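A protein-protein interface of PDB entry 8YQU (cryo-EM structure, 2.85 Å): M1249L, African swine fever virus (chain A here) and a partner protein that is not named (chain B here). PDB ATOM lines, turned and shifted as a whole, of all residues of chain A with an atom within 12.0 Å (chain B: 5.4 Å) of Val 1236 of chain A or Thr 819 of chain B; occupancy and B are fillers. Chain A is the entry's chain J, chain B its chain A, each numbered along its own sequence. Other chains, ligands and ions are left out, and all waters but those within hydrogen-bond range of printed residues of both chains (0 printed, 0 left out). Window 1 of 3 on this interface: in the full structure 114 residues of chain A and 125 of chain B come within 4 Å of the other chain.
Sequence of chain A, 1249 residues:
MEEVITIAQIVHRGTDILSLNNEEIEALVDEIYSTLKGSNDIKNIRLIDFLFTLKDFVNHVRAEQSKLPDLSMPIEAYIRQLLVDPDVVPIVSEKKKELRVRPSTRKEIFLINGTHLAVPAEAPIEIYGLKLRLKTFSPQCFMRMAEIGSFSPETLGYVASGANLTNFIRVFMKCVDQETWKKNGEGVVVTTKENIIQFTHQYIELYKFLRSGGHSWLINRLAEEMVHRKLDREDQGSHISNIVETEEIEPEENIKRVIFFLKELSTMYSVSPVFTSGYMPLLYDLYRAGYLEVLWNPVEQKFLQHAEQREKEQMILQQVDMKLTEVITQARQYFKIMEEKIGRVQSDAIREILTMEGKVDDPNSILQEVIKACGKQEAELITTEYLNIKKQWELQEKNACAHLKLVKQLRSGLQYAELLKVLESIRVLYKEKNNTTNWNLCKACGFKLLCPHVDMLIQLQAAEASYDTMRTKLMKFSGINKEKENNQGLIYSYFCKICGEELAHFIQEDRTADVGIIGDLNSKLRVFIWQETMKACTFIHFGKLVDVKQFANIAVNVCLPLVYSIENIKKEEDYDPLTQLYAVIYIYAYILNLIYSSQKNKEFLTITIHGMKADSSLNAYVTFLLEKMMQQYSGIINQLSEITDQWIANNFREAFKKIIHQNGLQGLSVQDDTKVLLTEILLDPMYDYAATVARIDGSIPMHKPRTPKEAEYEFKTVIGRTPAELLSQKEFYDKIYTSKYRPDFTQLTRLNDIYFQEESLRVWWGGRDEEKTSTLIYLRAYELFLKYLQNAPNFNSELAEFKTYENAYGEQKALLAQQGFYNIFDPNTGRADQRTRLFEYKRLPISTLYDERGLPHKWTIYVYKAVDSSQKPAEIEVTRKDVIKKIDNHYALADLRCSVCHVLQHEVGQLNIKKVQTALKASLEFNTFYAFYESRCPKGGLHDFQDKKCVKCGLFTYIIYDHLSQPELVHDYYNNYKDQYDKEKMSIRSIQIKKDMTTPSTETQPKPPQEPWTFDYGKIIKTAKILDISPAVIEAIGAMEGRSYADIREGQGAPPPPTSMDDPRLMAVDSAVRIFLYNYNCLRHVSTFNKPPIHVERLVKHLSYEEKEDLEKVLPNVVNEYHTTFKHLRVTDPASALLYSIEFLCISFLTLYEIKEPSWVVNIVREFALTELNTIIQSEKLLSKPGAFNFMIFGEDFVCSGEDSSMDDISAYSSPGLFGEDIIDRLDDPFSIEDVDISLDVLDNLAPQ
NZ of Lys 306 of chain B lies within hydrogen-bond range of O of Ile 1233 of chain A, 3.4 Å away.
The side-chain amino group of Lys 306 of chain B sits at hydrogen-bond distance from the backbone carbonyl oxygen of Val 1236 of chain A, at 2.6 Å.
The guanidinium group (NH2) of Arg 311 of chain B lies within hydrogen-bond range of the backbone carbonyl oxygen (O) of Glu 1234 of chain A, at 2.5 Å.
OD1 of Asp 1235 of chain A lies within salt-bridge range of NH1 of Arg 311 of chain B (2.9 Å).
O of Leu 1246 of chain A lies within hydrogen-bond range of NZ of Lys 815 of chain B.
The side-chain hydroxyl (OH) of Tyr 824 of chain B sits at hydrogen-bond distance from the backbone carbonyl oxygen (O) of Asp 1229 of chain A, at 3.2 Å.
The side-chain hydroxyl (OH) of Tyr 824 of chain B sits at hydrogen-bond distance from the side-chain hydroxyl (OG) of Ser 1232 of chain A (2.6 Å).
The backbone carbonyl oxygen (O) of Pro 1230 of chain A lies close to the side-chain hydroxyl (OG) of Ser 820 of chain B (2.3 Å).
The side-chain carboxylate (OD2) of Asp 1229 of chain A sits close to the backbone NH (N) of Phe 1231 of chain A (3.3 Å).
The side-chain hydroxyl of Ser 1232 of chain A is in hydrogen-bond range of the backbone carbonyl oxygen of Asp 1229 of chain A, 3.1 Å away.
Among the printed residues, merely in contact across the chains: Pro 1230 of chain A with Leu 817 of chain B, Pro 1230 of chain A with Ser 821 of chain B, Phe 1231 of chain A with Ala 816 of chain B, Phe 1231 of chain A with Leu 817 of chain B, Phe 1231 of chain A with Ser 820 of chain B, Ser 1232 of chain A with Ser 820 of chain B, Ile 1233 of chain A with Thr 819 of chain B, Glu 1234 of chain A with Lys 306 of chain B, Glu 1234 of chain A with Tyr 824 of chain B, Asp 1235 of chain A with Gly 823 of chain B, Asp 1235 of chain A with Tyr 824 of chain B, Val 1236 of chain A with Thr 819 of chain B, Val 1236 of chain A with Gly 823 of chain B, Leu 1246 of chain A with Pro 421 of chain B, Leu 1246 of chain A with Thr 819 of chain B and Pro 1248 of chain A with Lys 815 of chain B.
Of chain B, only Lys 306, Thr 819 and Gly 823 come within 4 Å of Val 1236 of chain A.
Pro 421 of chain B touches just one residue of chain A: Leu 1246 (3.9 Å).
No residue of chain A comes within 4 Å of Ser 818 of chain B.
Ser 820 of chain B touches three residues of chain A.
Of the printed residues of chain B, Pro 1230 of chain A touches Leu 817, Ser 820 and Ser 821.
Of the printed residues of chain A, Arg 311 of chain B touches Glu 1234 and Asp 1235.
Ser 1239 of chain A touches none of the printed residues of chain B.
The nearest printed residue of chain B that does not touch Asp 1229 of chain A is Ser 820 of chain B (5.1 Å).
Printed residues of chain A that touch a printed residue of chain B: Asp 1229, Pro 1230, Phe 1231, Ser 1232, Ile 1233, Glu 1234, Asp 1235, Val 1236, Leu 1246 and Pro 1248.
Hydrophobic or aromatic side chains of chain A that line the printed part of chain B: Phe 1231, Ile 1233, Val 1236, Leu 1246 and Pro 1248.
Of the 14 printed residues of chain B, 11 touch a printed residue of chain A.
Hydrophobic or aromatic side chains of chain B within 4 Å of the printed part of chain A: Pro 421, Ala 816, Leu 817 and Tyr 824.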
ATOM      1  N   ASP A1228     -35.636 -25.778 -16.918  1.00  0.00           N
ATOM      2  CA  ASP A1228     -34.738 -25.270 -17.945  1.00  0.00           C
ATOM      3  C   ASP A1228     -34.881 -23.759 -18.075  1.00  0.00           C
ATOM      4  O   ASP A1228     -35.993 -23.225 -18.082  1.00  0.00           O
ATOM      5  CB  ASP A1228     -35.024 -25.934 -19.293  1.00  0.00           C
ATOM      6  CG  ASP A1228     -34.635 -27.397 -19.316  1.00  0.00           C
ATOM      7  OD1 ASP A1228     -33.696 -27.776 -18.587  1.00  0.00           O
ATOM      8  OD2 ASP A1228     -35.269 -28.169 -20.066  1.00  0.00           O
ATOM      9  N   ASP A1229     -33.747 -23.077 -18.175  1.00  0.00           N
ATOM     10  CA  ASP A1229     -33.756 -21.643 -18.423  1.00  0.00           C
ATOM     11  C   ASP A1229     -34.003 -21.393 -19.905  1.00  0.00           C
ATOM     12  O   ASP A1229     -33.187 -21.810 -20.735  1.00  0.00           O
ATOM     13  CB  ASP A1229     -32.436 -21.016 -17.994  1.00  0.00           C
ATOM     14  CG  ASP A1229     -32.504 -19.504 -17.918  1.00  0.00           C
ATOM     15  OD1 ASP A1229     -33.019 -18.980 -16.908  1.00  0.00           O
ATOM     16  OD2 ASP A1229     -32.042 -18.839 -18.868  1.00  0.00           O
ATOM     17  N   PRO A1230     -35.102 -20.737 -20.282  1.00  0.00           N
ATOM     18  CA  PRO A1230     -35.394 -20.557 -21.713  1.00  0.00           C
ATOM     19  C   PRO A1230     -34.394 -19.677 -22.441  1.00  0.00           C
ATOM     20  O   PRO A1230     -34.275 -19.794 -23.667  1.00  0.00           O
ATOM     21  CB  PRO A1230     -36.792 -19.926 -21.709  1.00  0.00           C
ATOM     22  CG  PRO A1230     -36.893 -19.249 -20.385  1.00  0.00           C
ATOM     23  CD  PRO A1230     -36.117 -20.103 -19.423  1.00  0.00           C
ATOM     24  N   PHE A1231     -33.669 -18.811 -21.735  1.00  0.00           N
ATOM     25  CA  PHE A1231     -32.770 -17.853 -22.362  1.00  0.00           C
ATOM     26  C   PHE A1231     -31.306 -18.257 -22.262  1.00  0.00           C
ATOM     27  O   PHE A1231     -30.432 -17.471 -22.639  1.00  0.00           O
ATOM     28  CB  PHE A1231     -32.969 -16.468 -21.743  1.00  0.00           C
ATOM     29  CG  PHE A1231     -34.172 -15.739 -22.264  1.00  0.00           C
ATOM     30  CD1 PHE A1231     -35.424 -15.973 -21.723  1.00  0.00           C
ATOM     31  CD2 PHE A1231     -34.054 -14.827 -23.297  1.00  0.00           C
ATOM     32  CE1 PHE A1231     -36.535 -15.306 -22.198  1.00  0.00           C
ATOM     33  CE2 PHE A1231     -35.160 -14.158 -23.777  1.00  0.00           C
ATOM     34  CZ  PHE A1231     -36.403 -14.399 -23.228  1.00  0.00           C
ATOM     35  N   SER A1232     -31.016 -19.458 -21.771  1.00  0.00           N
ATOM     36  CA  SER A1232     -29.646 -19.904 -21.563  1.00  0.00           C
ATOM     37  C   SER A1232     -29.212 -20.807 -22.710  1.00  0.00           C
ATOM     38  O   SER A1232     -29.907 -21.772 -23.043  1.00  0.00           O
ATOM     39  CB  SER A1232     -29.510 -20.646 -20.233  1.00  0.00           C
ATOM     40  OG  SER A1232     -30.098 -21.933 -20.307  1.00  0.00           O
ATOM     41  N   ILE A1233     -28.064 -20.494 -23.302  1.00  0.00           N
ATOM     42  CA  ILE A1233     -27.489 -21.336 -24.364  1.00  0.00           C
ATOM     43  C   ILE A1233     -26.662 -22.408 -23.661  1.00  0.00           C
ATOM     44  O   ILE A1233     -25.460 -22.280 -23.418  1.00  0.00           O
ATOM     45  CB  ILE A1233     -26.702 -20.512 -25.397  1.00  0.00           C
ATOM     46  CG1 ILE A1233     -25.532 -19.749 -24.765  1.00  0.00           C
ATOM     47  CG2 ILE A1233     -27.626 -19.542 -26.119  1.00  0.00           C
ATOM     48  CD1 ILE A1233     -24.602 -19.116 -25.773  1.00  0.00           C
ATOM     49  N   GLU A1234     -27.334 -23.504 -23.314  1.00  0.00           N
ATOM     50  CA  GLU A1234     -26.695 -24.621 -22.630  1.00  0.00           C
ATOM     51  C   GLU A1234     -26.504 -25.833 -23.529  1.00  0.00           C
ATOM     52  O   GLU A1234     -25.520 -26.562 -23.377  1.00  0.00           O
ATOM     53  CB  GLU A1234     -27.507 -25.023 -21.394  1.00  0.00           C
ATOM     54  CG  GLU A1234     -26.796 -26.003 -20.471  1.00  0.00           C
ATOM     55  CD  GLU A1234     -25.661 -25.360 -19.691  1.00  0.00           C
ATOM     56  OE1 GLU A1234     -25.581 -24.114 -19.663  1.00  0.00           O
ATOM     57  OE2 GLU A1234     -24.849 -26.104 -19.103  1.00  0.00           O
ATOM     58  N   ASP A1235     -27.421 -26.072 -24.465  1.00  0.00           N
ATOM     59  CA  ASP A1235     -27.241 -27.098 -25.479  1.00  0.00           C
ATOM     60  C   ASP A1235     -26.778 -26.522 -26.809  1.00  0.00           C
ATOM     61  O   ASP A1235     -26.732 -27.248 -27.808  1.00  0.00           O
ATOM     62  CB  ASP A1235     -28.529 -27.901 -25.664  1.00  0.00           C
ATOM     63  CG  ASP A1235     -28.897 -28.705 -24.429  1.00  0.00           C
ATOM     64  OD1 ASP A1235     -27.987 -29.031 -23.638  1.00  0.00           O
ATOM     65  OD2 ASP A1235     -30.090 -29.032 -24.261  1.00  0.00           O
ATOM     66  N   VAL A1236     -26.437 -25.238 -26.846  1.00  0.00           N
ATOM     67  CA  VAL A1236     -25.856 -24.605 -28.022  1.00  0.00           C
ATOM     68  C   VAL A1236     -24.354 -24.509 -27.797  1.00  0.00           C
ATOM     69  O   VAL A1236     -23.898 -23.795 -26.896  1.00  0.00           O
ATOM     70  CB  VAL A1236     -26.465 -23.219 -28.277  1.00  0.00           C
ATOM     71  CG1 VAL A1236     -25.798 -22.559 -29.473  1.00  0.00           C
ATOM     72  CG2 VAL A1236     -27.962 -23.327 -28.488  1.00  0.00           C
ATOM     73  N   ASP A1237     -23.584 -25.223 -28.613  1.00  0.00           N
ATOM     74  CA  ASP A1237     -22.130 -25.265 -28.477  1.00  0.00           C
ATOM     75  C   ASP A1237     -21.543 -24.195 -29.391  1.00  0.00           C
ATOM     76  O   ASP A1237     -21.201 -24.453 -30.546  1.00  0.00           O
ATOM     77  CB  ASP A1237     -21.590 -26.652 -28.800  1.00  0.00           C
ATOM     78  CG  ASP A1237     -20.275 -26.939 -28.104  1.00  0.00           C
ATOM     79  OD1 ASP A1237     -19.735 -26.023 -27.450  1.00  0.00           O
ATOM     80  OD2 ASP A1237     -19.783 -28.082 -28.205  1.00  0.00           O
ATOM     81  N   ILE A1238     -21.435 -22.979 -28.863  1.00  0.00           N
ATOM     82  CA  ILE A1238     -20.831 -21.853 -29.561  1.00  0.00           C
ATOM     83  C   ILE A1238     -19.855 -21.181 -28.607  1.00  0.00           C
ATOM     84  O   ILE A1238     -20.140 -21.034 -27.414  1.00  0.00           O
ATOM     85  CB  ILE A1238     -21.897 -20.855 -30.067  1.00  0.00           C
ATOM     86  CG1 ILE A1238     -21.240 -19.611 -30.668  1.00  0.00           C
ATOM     87  CG2 ILE A1238     -22.850 -20.469 -28.948  1.00  0.00           C
ATOM     88  CD1 ILE A1238     -22.194 -18.737 -31.445  1.00  0.00           C
ATOM     89  N   SER A1239     -18.691 -20.796 -29.128  1.00  0.00           N
ATOM     90  CA  SER A1239     -17.666 -20.187 -28.293  1.00  0.00           C
ATOM     91  C   SER A1239     -18.160 -18.871 -27.706  1.00  0.00           C
ATOM     92  O   SER A1239     -18.889 -18.117 -28.354  1.00  0.00           O
ATOM     93  CB  SER A1239     -16.390 -19.958 -29.101  1.00  0.00           C
ATOM     94  OG  SER A1239     -15.464 -19.168 -28.378  1.00  0.00           O
ATOM     95  N   LEU A1240     -17.754 -18.599 -26.464  1.00  0.00           N
ATOM     96  CA  LEU A1240     -18.190 -17.383 -25.787  1.00  0.00           C
ATOM     97  C   LEU A1240     -17.527 -16.134 -26.352  1.00  0.00           C
ATOM     98  O   LEU A1240     -17.982 -15.022 -26.061  1.00  0.00           O
ATOM     99  CB  LEU A1240     -17.912 -17.481 -24.284  1.00  0.00           C
ATOM    100  CG  LEU A1240     -18.922 -18.208 -23.386  1.00  0.00           C
ATOM    101  CD1 LEU A1240     -20.262 -17.488 -23.392  1.00  0.00           C
ATOM    102  CD2 LEU A1240     -19.092 -19.674 -23.766  1.00  0.00           C
ATOM    103  N   ASP A1241     -16.471 -16.288 -27.144  1.00  0.00           N
ATOM    104  CA  ASP A1241     -15.777 -15.160 -27.748  1.00  0.00           C
ATOM    105  C   ASP A1241     -16.298 -14.817 -29.136  1.00  0.00           C
ATOM    106  O   ASP A1241     -15.803 -13.867 -29.751  1.00  0.00           O
ATOM    107  CB  ASP A1241     -14.273 -15.446 -27.822  1.00  0.00           C
ATOM    108  CG  ASP A1241     -13.586 -15.303 -26.480  1.00  0.00           C
ATOM    109  OD1 ASP A1241     -14.103 -14.559 -25.622  1.00  0.00           O
ATOM    110  OD2 ASP A1241     -12.528 -15.937 -26.282  1.00  0.00           O
ATOM    111  N   VAL A1242     -17.280 -15.560 -29.642  1.00  0.00           N
ATOM    112  CA  VAL A1242     -17.795 -15.351 -30.990  1.00  0.00           C
ATOM    113  C   VAL A1242     -19.311 -15.207 -30.899  1.00  0.00           C
ATOM    114  O   VAL A1242     -20.050 -15.544 -31.831  1.00  0.00           O
ATOM    115  CB  VAL A1242     -17.357 -16.503 -31.920  1.00  0.00           C
ATOM    116  CG1 VAL A1242     -18.018 -17.822 -31.524  1.00  0.00           C
ATOM    117  CG2 VAL A1242     -17.571 -16.158 -33.390  1.00  0.00           C
ATOM    118  N   LEU A1243     -19.788 -14.684 -29.767  1.00  0.00           N
ATOM    119  CA  LEU A1243     -21.221 -14.560 -29.527  1.00  0.00           C
ATOM    120  C   LEU A1243     -21.895 -13.527 -30.420  1.00  0.00           C
ATOM    121  O   LEU A1243     -23.129 -13.483 -30.455  1.00  0.00           O
ATOM    122  CB  LEU A1243     -21.479 -14.210 -28.061  1.00  0.00           C
ATOM    123  CG  LEU A1243     -21.245 -15.321 -27.038  1.00  0.00           C
ATOM    124  CD1 LEU A1243     -21.455 -14.792 -25.631  1.00  0.00           C
ATOM    125  CD2 LEU A1243     -22.160 -16.504 -27.312  1.00  0.00           C
ATOM    126  N   ASP A1244     -21.132 -12.697 -31.133  1.00  0.00           N
ATOM    127  CA  ASP A1244     -21.737 -11.699 -32.006  1.00  0.00           C
ATOM    128  C   ASP A1244     -22.415 -12.308 -33.226  1.00  0.00           C
ATOM    129  O   ASP A1244     -23.154 -11.598 -33.915  1.00  0.00           O
ATOM    130  CB  ASP A1244     -20.689 -10.681 -32.454  1.00  0.00           C
ATOM    131  CG  ASP A1244     -20.443  -9.606 -31.417  1.00  0.00           C
ATOM    132  OD1 ASP A1244     -21.117  -9.628 -30.365  1.00  0.00           O
ATOM    133  OD2 ASP A1244     -19.578  -8.736 -31.652  1.00  0.00           O
ATOM    134  N   ASN A1245     -22.186 -13.592 -33.513  1.00  0.00           N
ATOM    135  CA  ASN A1245     -22.927 -14.251 -34.580  1.00  0.00           C
ATOM    136  C   ASN A1245     -24.404 -14.406 -34.251  1.00  0.00           C
ATOM    137  O   ASN A1245     -25.201 -14.660 -35.159  1.00  0.00           O
ATOM    138  CB  ASN A1245     -22.329 -15.626 -34.880  1.00  0.00           C
ATOM    139  CG  ASN A1245     -20.851 -15.563 -35.191  1.00  0.00           C
ATOM    140  OD1 ASN A1245     -20.298 -14.490 -35.426  1.00  0.00           O
ATOM    141  ND2 ASN A1245     -20.205 -16.721 -35.212  1.00  0.00           N
ATOM    142  N   LEU A1246     -24.782 -14.262 -32.983  1.00  0.00           N
ATOM    143  CA  LEU A1246     -26.167 -14.356 -32.551  1.00  0.00           C
ATOM    144  C   LEU A1246     -26.854 -13.000 -32.513  1.00  0.00           C
ATOM    145  O   LEU A1246     -28.004 -12.911 -32.072  1.00  0.00           O
ATOM    146  CB  LEU A1246     -26.242 -15.020 -31.175  1.00  0.00           C
ATOM    147  CG  LEU A1246     -25.486 -16.339 -31.017  1.00  0.00           C
ATOM    148  CD1 LEU A1246     -25.611 -16.863 -29.597  1.00  0.00           C
ATOM    149  CD2 LEU A1246     -25.987 -17.368 -32.017  1.00  0.00           C
ATOM    150  N   ALA A1247     -26.175 -11.946 -32.955  1.00  0.00           N
ATOM    151  CA  ALA A1247     -26.779 -10.624 -32.967  1.00  0.00           C
ATOM    152  C   ALA A1247     -27.957 -10.596 -33.938  1.00  0.00           C
ATOM    153  O   ALA A1247     -27.882 -11.178 -35.025  1.00  0.00           O
ATOM    154  CB  ALA A1247     -25.751  -9.566 -33.359  1.00  0.00           C
ATOM    155  N   PRO A1248     -29.062  -9.940 -33.571  1.00  0.00           N
ATOM    156  CA  PRO A1248     -30.227  -9.910 -34.468  1.00  0.00           C
ATOM    157  C   PRO A1248     -29.946  -9.268 -35.813  1.00  0.00           C
ATOM    158  O   PRO A1248     -30.535  -9.686 -36.819  1.00  0.00           O
ATOM    159  CB  PRO A1248     -31.265  -9.114 -33.664  1.00  0.00           C
ATOM    160  CG  PRO A1248     -30.468  -8.330 -32.676  1.00  0.00           C
ATOM    161  CD  PRO A1248     -29.288  -9.178 -32.334  1.00  0.00           C
ATOM    162  N   GLN A1249     -29.065  -8.270 -35.862  1.00  0.00           N
ATOM    163  CA  GLN A1249     -28.717  -7.576 -37.101  1.00  0.00           C
ATOM    164  C   GLN A1249     -29.950  -7.041 -37.821  1.00  0.00           C
ATOM    165  O   GLN A1249     -29.910  -5.974 -38.432  1.00  0.00           O
ATOM    166  CB  GLN A1249     -27.929  -8.500 -38.034  1.00  0.00           C
ATOM    167  CG  GLN A1249     -27.533  -7.856 -39.354  1.00  0.00           C
ATOM    168  CD  GLN A1249     -28.399  -8.319 -40.510  1.00  0.00           C
ATOM    169  OE1 GLN A1249     -29.002  -9.391 -40.459  1.00  0.00           O
ATOM    170  NE2 GLN A1249     -28.463  -7.512 -41.563  1.00  0.00           N
ATOM    171  N   LYS B 306     -22.567 -29.038 -19.342  1.00  0.00           N
ATOM    172  CA  LYS B 306     -21.930 -28.658 -20.599  1.00  0.00           C
ATOM    173  C   LYS B 306     -20.416 -28.593 -20.473  1.00  0.00           C
ATOM    174  O   LYS B 306     -19.700 -29.085 -21.351  1.00  0.00           O
ATOM    175  CB  LYS B 306     -22.467 -27.307 -21.068  1.00  0.00           C
ATOM    176  CG  LYS B 306     -21.935 -26.855 -22.416  1.00  0.00           C
ATOM    177  CD  LYS B 306     -22.569 -25.541 -22.834  1.00  0.00           C
ATOM    178  CE  LYS B 306     -22.044 -25.072 -24.177  1.00  0.00           C
ATOM    179  NZ  LYS B 306     -22.660 -23.780 -24.586  1.00  0.00           N
ATOM    180  N   ARG B 311     -19.377 -33.636 -22.571  1.00  0.00           N
ATOM    181  CA  ARG B 311     -19.776 -32.653 -23.567  1.00  0.00           C
ATOM    182  C   ARG B 311     -18.674 -31.669 -23.932  1.00  0.00           C
ATOM    183  O   ARG B 311     -18.795 -30.982 -24.954  1.00  0.00           O
ATOM    184  CB  ARG B 311     -21.002 -31.876 -23.081  1.00  0.00           C
ATOM    185  CG  ARG B 311     -22.287 -32.682 -23.101  1.00  0.00           C
ATOM    186  CD  ARG B 311     -23.478 -31.814 -22.750  1.00  0.00           C
ATOM    187  NE  ARG B 311     -23.560 -30.646 -23.618  1.00  0.00           N
ATOM    188  CZ  ARG B 311     -24.456 -29.678 -23.489  1.00  0.00           C
ATOM    189  NH1 ARG B 311     -25.370 -29.706 -22.534  1.00  0.00           N
ATOM    190  NH2 ARG B 311     -24.433 -28.657 -24.339  1.00  0.00           N
ATOM    191  N   PRO B 421     -23.350 -20.752 -34.814  1.00  0.00           N
ATOM    192  CA  PRO B 421     -23.618 -22.183 -34.599  1.00  0.00           C
ATOM    193  C   PRO B 421     -23.726 -22.961 -35.906  1.00  0.00           C
ATOM    194  O   PRO B 421     -24.139 -22.421 -36.927  1.00  0.00           O
ATOM    195  CB  PRO B 421     -24.947 -22.170 -33.834  1.00  0.00           C
ATOM    196  CG  PRO B 421     -25.637 -20.934 -34.319  1.00  0.00           C
ATOM    197  CD  PRO B 421     -24.537 -19.926 -34.530  1.00  0.00           C
ATOM    198  N   ASN B 814     -37.634 -12.627 -28.838  1.00  0.00           N
ATOM    199  CA  ASN B 814     -37.797 -13.860 -29.599  1.00  0.00           C
ATOM    200  C   ASN B 814     -36.528 -14.227 -30.357  1.00  0.00           C
ATOM    201  O   ASN B 814     -36.270 -15.413 -30.589  1.00  0.00           O
ATOM    202  CB  ASN B 814     -38.974 -13.733 -30.565  1.00  0.00           C
ATOM    203  CG  ASN B 814     -40.306 -13.661 -29.850  1.00  0.00           C
ATOM    204  OD1 ASN B 814     -41.129 -12.792 -30.131  1.00  0.00           O
ATOM    205  ND2 ASN B 814     -40.523 -14.574 -28.913  1.00  0.00           N
ATOM    206  N   LYS B 815     -35.733 -13.234 -30.760  1.00  0.00           N
ATOM    207  CA  LYS B 815     -34.453 -13.531 -31.393  1.00  0.00           C
ATOM    208  C   LYS B 815     -33.509 -14.226 -30.421  1.00  0.00           C
ATOM    209  O   LYS B 815     -32.792 -15.159 -30.802  1.00  0.00           O
ATOM    210  CB  LYS B 815     -33.821 -12.251 -31.935  1.00  0.00           C
ATOM    211  CG  LYS B 815     -32.468 -12.466 -32.587  1.00  0.00           C
ATOM    212  CD  LYS B 815     -32.599 -13.271 -33.866  1.00  0.00           C
ATOM    213  CE  LYS B 815     -31.241 -13.568 -34.479  1.00  0.00           C
ATOM    214  NZ  LYS B 815     -30.492 -14.587 -33.695  1.00  0.00           N
ATOM    215  N   ALA B 816     -33.492 -13.782 -29.163  1.00  0.00           N
ATOM    216  CA  ALA B 816     -32.681 -14.453 -28.153  1.00  0.00           C
ATOM    217  C   ALA B 816     -33.171 -15.874 -27.909  1.00  0.00           C
ATOM    218  O   ALA B 816     -32.366 -16.800 -27.755  1.00  0.00           O
ATOM    219  CB  ALA B 816     -32.689 -13.650 -26.854  1.00  0.00           C
ATOM    220  N   LEU B 817     -34.492 -16.066 -27.870  1.00  0.00           N
ATOM    221  CA  LEU B 817     -35.041 -17.403 -27.679  1.00  0.00           C
ATOM    222  C   LEU B 817     -34.826 -18.285 -28.900  1.00  0.00           C
ATOM    223  O   LEU B 817     -34.735 -19.510 -28.766  1.00  0.00           O
ATOM    224  CB  LEU B 817     -36.528 -17.320 -27.342  1.00  0.00           C
ATOM    225  CG  LEU B 817     -36.857 -16.681 -25.995  1.00  0.00           C
ATOM    226  CD1 LEU B 817     -38.355 -16.516 -25.827  1.00  0.00           C
ATOM    227  CD2 LEU B 817     -36.288 -17.539 -24.885  1.00  0.00           C
ATOM    228  N   SER B 818     -34.729 -17.693 -30.090  1.00  0.00           N
ATOM    229  CA  SER B 818     -34.532 -18.477 -31.304  1.00  0.00           C
ATOM    230  C   SER B 818     -33.188 -19.188 -31.335  1.00  0.00           C
ATOM    231  O   SER B 818     -32.966 -20.013 -32.227  1.00  0.00           O
ATOM    232  CB  SER B 818     -34.671 -17.584 -32.537  1.00  0.00           C
ATOM    233  OG  SER B 818     -33.557 -16.720 -32.668  1.00  0.00           O
ATOM    234  N   THR B 819     -32.291 -18.888 -30.397  1.00  0.00           N
ATOM    235  CA  THR B 819     -31.020 -19.585 -30.268  1.00  0.00           C
ATOM    236  C   THR B 819     -31.059 -20.662 -29.190  1.00  0.00           C
ATOM    237  O   THR B 819     -30.755 -21.825 -29.465  1.00  0.00           O
ATOM    238  CB  THR B 819     -29.899 -18.585 -29.959  1.00  0.00           C
ATOM    239  OG1 THR B 819     -29.906 -17.539 -30.938  1.00  0.00           O
ATOM    240  CG2 THR B 819     -28.548 -19.280 -29.978  1.00  0.00           C
ATOM    241  N   SER B 820     -31.433 -20.292 -27.963  1.00  0.00           N
ATOM    242  CA  SER B 820     -31.427 -21.252 -26.864  1.00  0.00           C
ATOM    243  C   SER B 820     -32.537 -22.285 -27.017  1.00  0.00           C
ATOM    244  O   SER B 820     -32.295 -23.491 -26.887  1.00  0.00           O
ATOM    245  CB  SER B 820     -31.556 -20.515 -25.531  1.00  0.00           C
ATOM    246  OG  SER B 820     -32.804 -19.853 -25.435  1.00  0.00           O
ATOM    247  N   SER B 821     -33.763 -21.834 -27.297  1.00  0.00           N
ATOM    248  CA  SER B 821     -34.884 -22.765 -27.406  1.00  0.00           C
ATOM    249  C   SER B 821     -34.703 -23.714 -28.584  1.00  0.00           C
ATOM    250  O   SER B 821     -35.032 -24.901 -28.490  1.00  0.00           O
ATOM    251  CB  SER B 821     -36.200 -21.999 -27.532  1.00  0.00           C
ATOM    252  OG  SER B 821     -36.469 -21.250 -26.359  1.00  0.00           O
ATOM    253  N   THR B 822     -34.193 -23.205 -29.706  1.00  0.00           N
ATOM    254  CA  THR B 822     -33.892 -24.077 -30.836  1.00  0.00           C
ATOM    255  C   THR B 822     -32.773 -25.051 -30.492  1.00  0.00           C
ATOM    256  O   THR B 822     -32.811 -26.219 -30.899  1.00  0.00           O
ATOM    257  CB  THR B 822     -33.519 -23.242 -32.060  1.00  0.00           C
ATOM    258  OG1 THR B 822     -34.587 -22.337 -32.365  1.00  0.00           O
ATOM    259  CG2 THR B 822     -33.265 -24.136 -33.263  1.00  0.00           C
ATOM    260  N   GLY B 823     -31.773 -24.593 -29.737  1.00  0.00           N
ATOM    261  CA  GLY B 823     -30.674 -25.470 -29.368  1.00  0.00           C
ATOM    262  C   GLY B 823     -31.100 -26.601 -28.453  1.00  0.00           C
ATOM    263  O   GLY B 823     -30.568 -27.711 -28.536  1.00  0.00           O
ATOM    264  N   TYR B 824     -32.053 -26.335 -27.556  1.00  0.00           N
ATOM    265  CA  TYR B 824     -32.573 -27.396 -26.700  1.00  0.00           C
ATOM    266  C   TYR B 824     -33.263 -28.475 -27.523  1.00  0.00           C
ATOM    267  O   TYR B 824     -33.093 -29.670 -27.261  1.00  0.00           O
ATOM    268  CB  TYR B 824     -33.539 -26.817 -25.665  1.00  0.00           C
ATOM    269  CG  TYR B 824     -32.869 -26.086 -24.521  1.00  0.00           C
ATOM    270  CD1 TYR B 824     -31.936 -26.723 -23.716  1.00  0.00           C
ATOM    271  CD2 TYR B 824     -33.182 -24.764 -24.237  1.00  0.00           C
ATOM    272  CE1 TYR B 824     -31.325 -26.061 -22.669  1.00  0.00           C
ATOM    273  CE2 TYR B 824     -32.577 -24.094 -23.192  1.00  0.00           C
ATOM    274  CZ  TYR B 824     -31.650 -24.747 -22.411  1.00  0.00           C
ATOM    275  OH  TYR B 824     -31.046 -24.085 -21.369  1.00  0.00           O
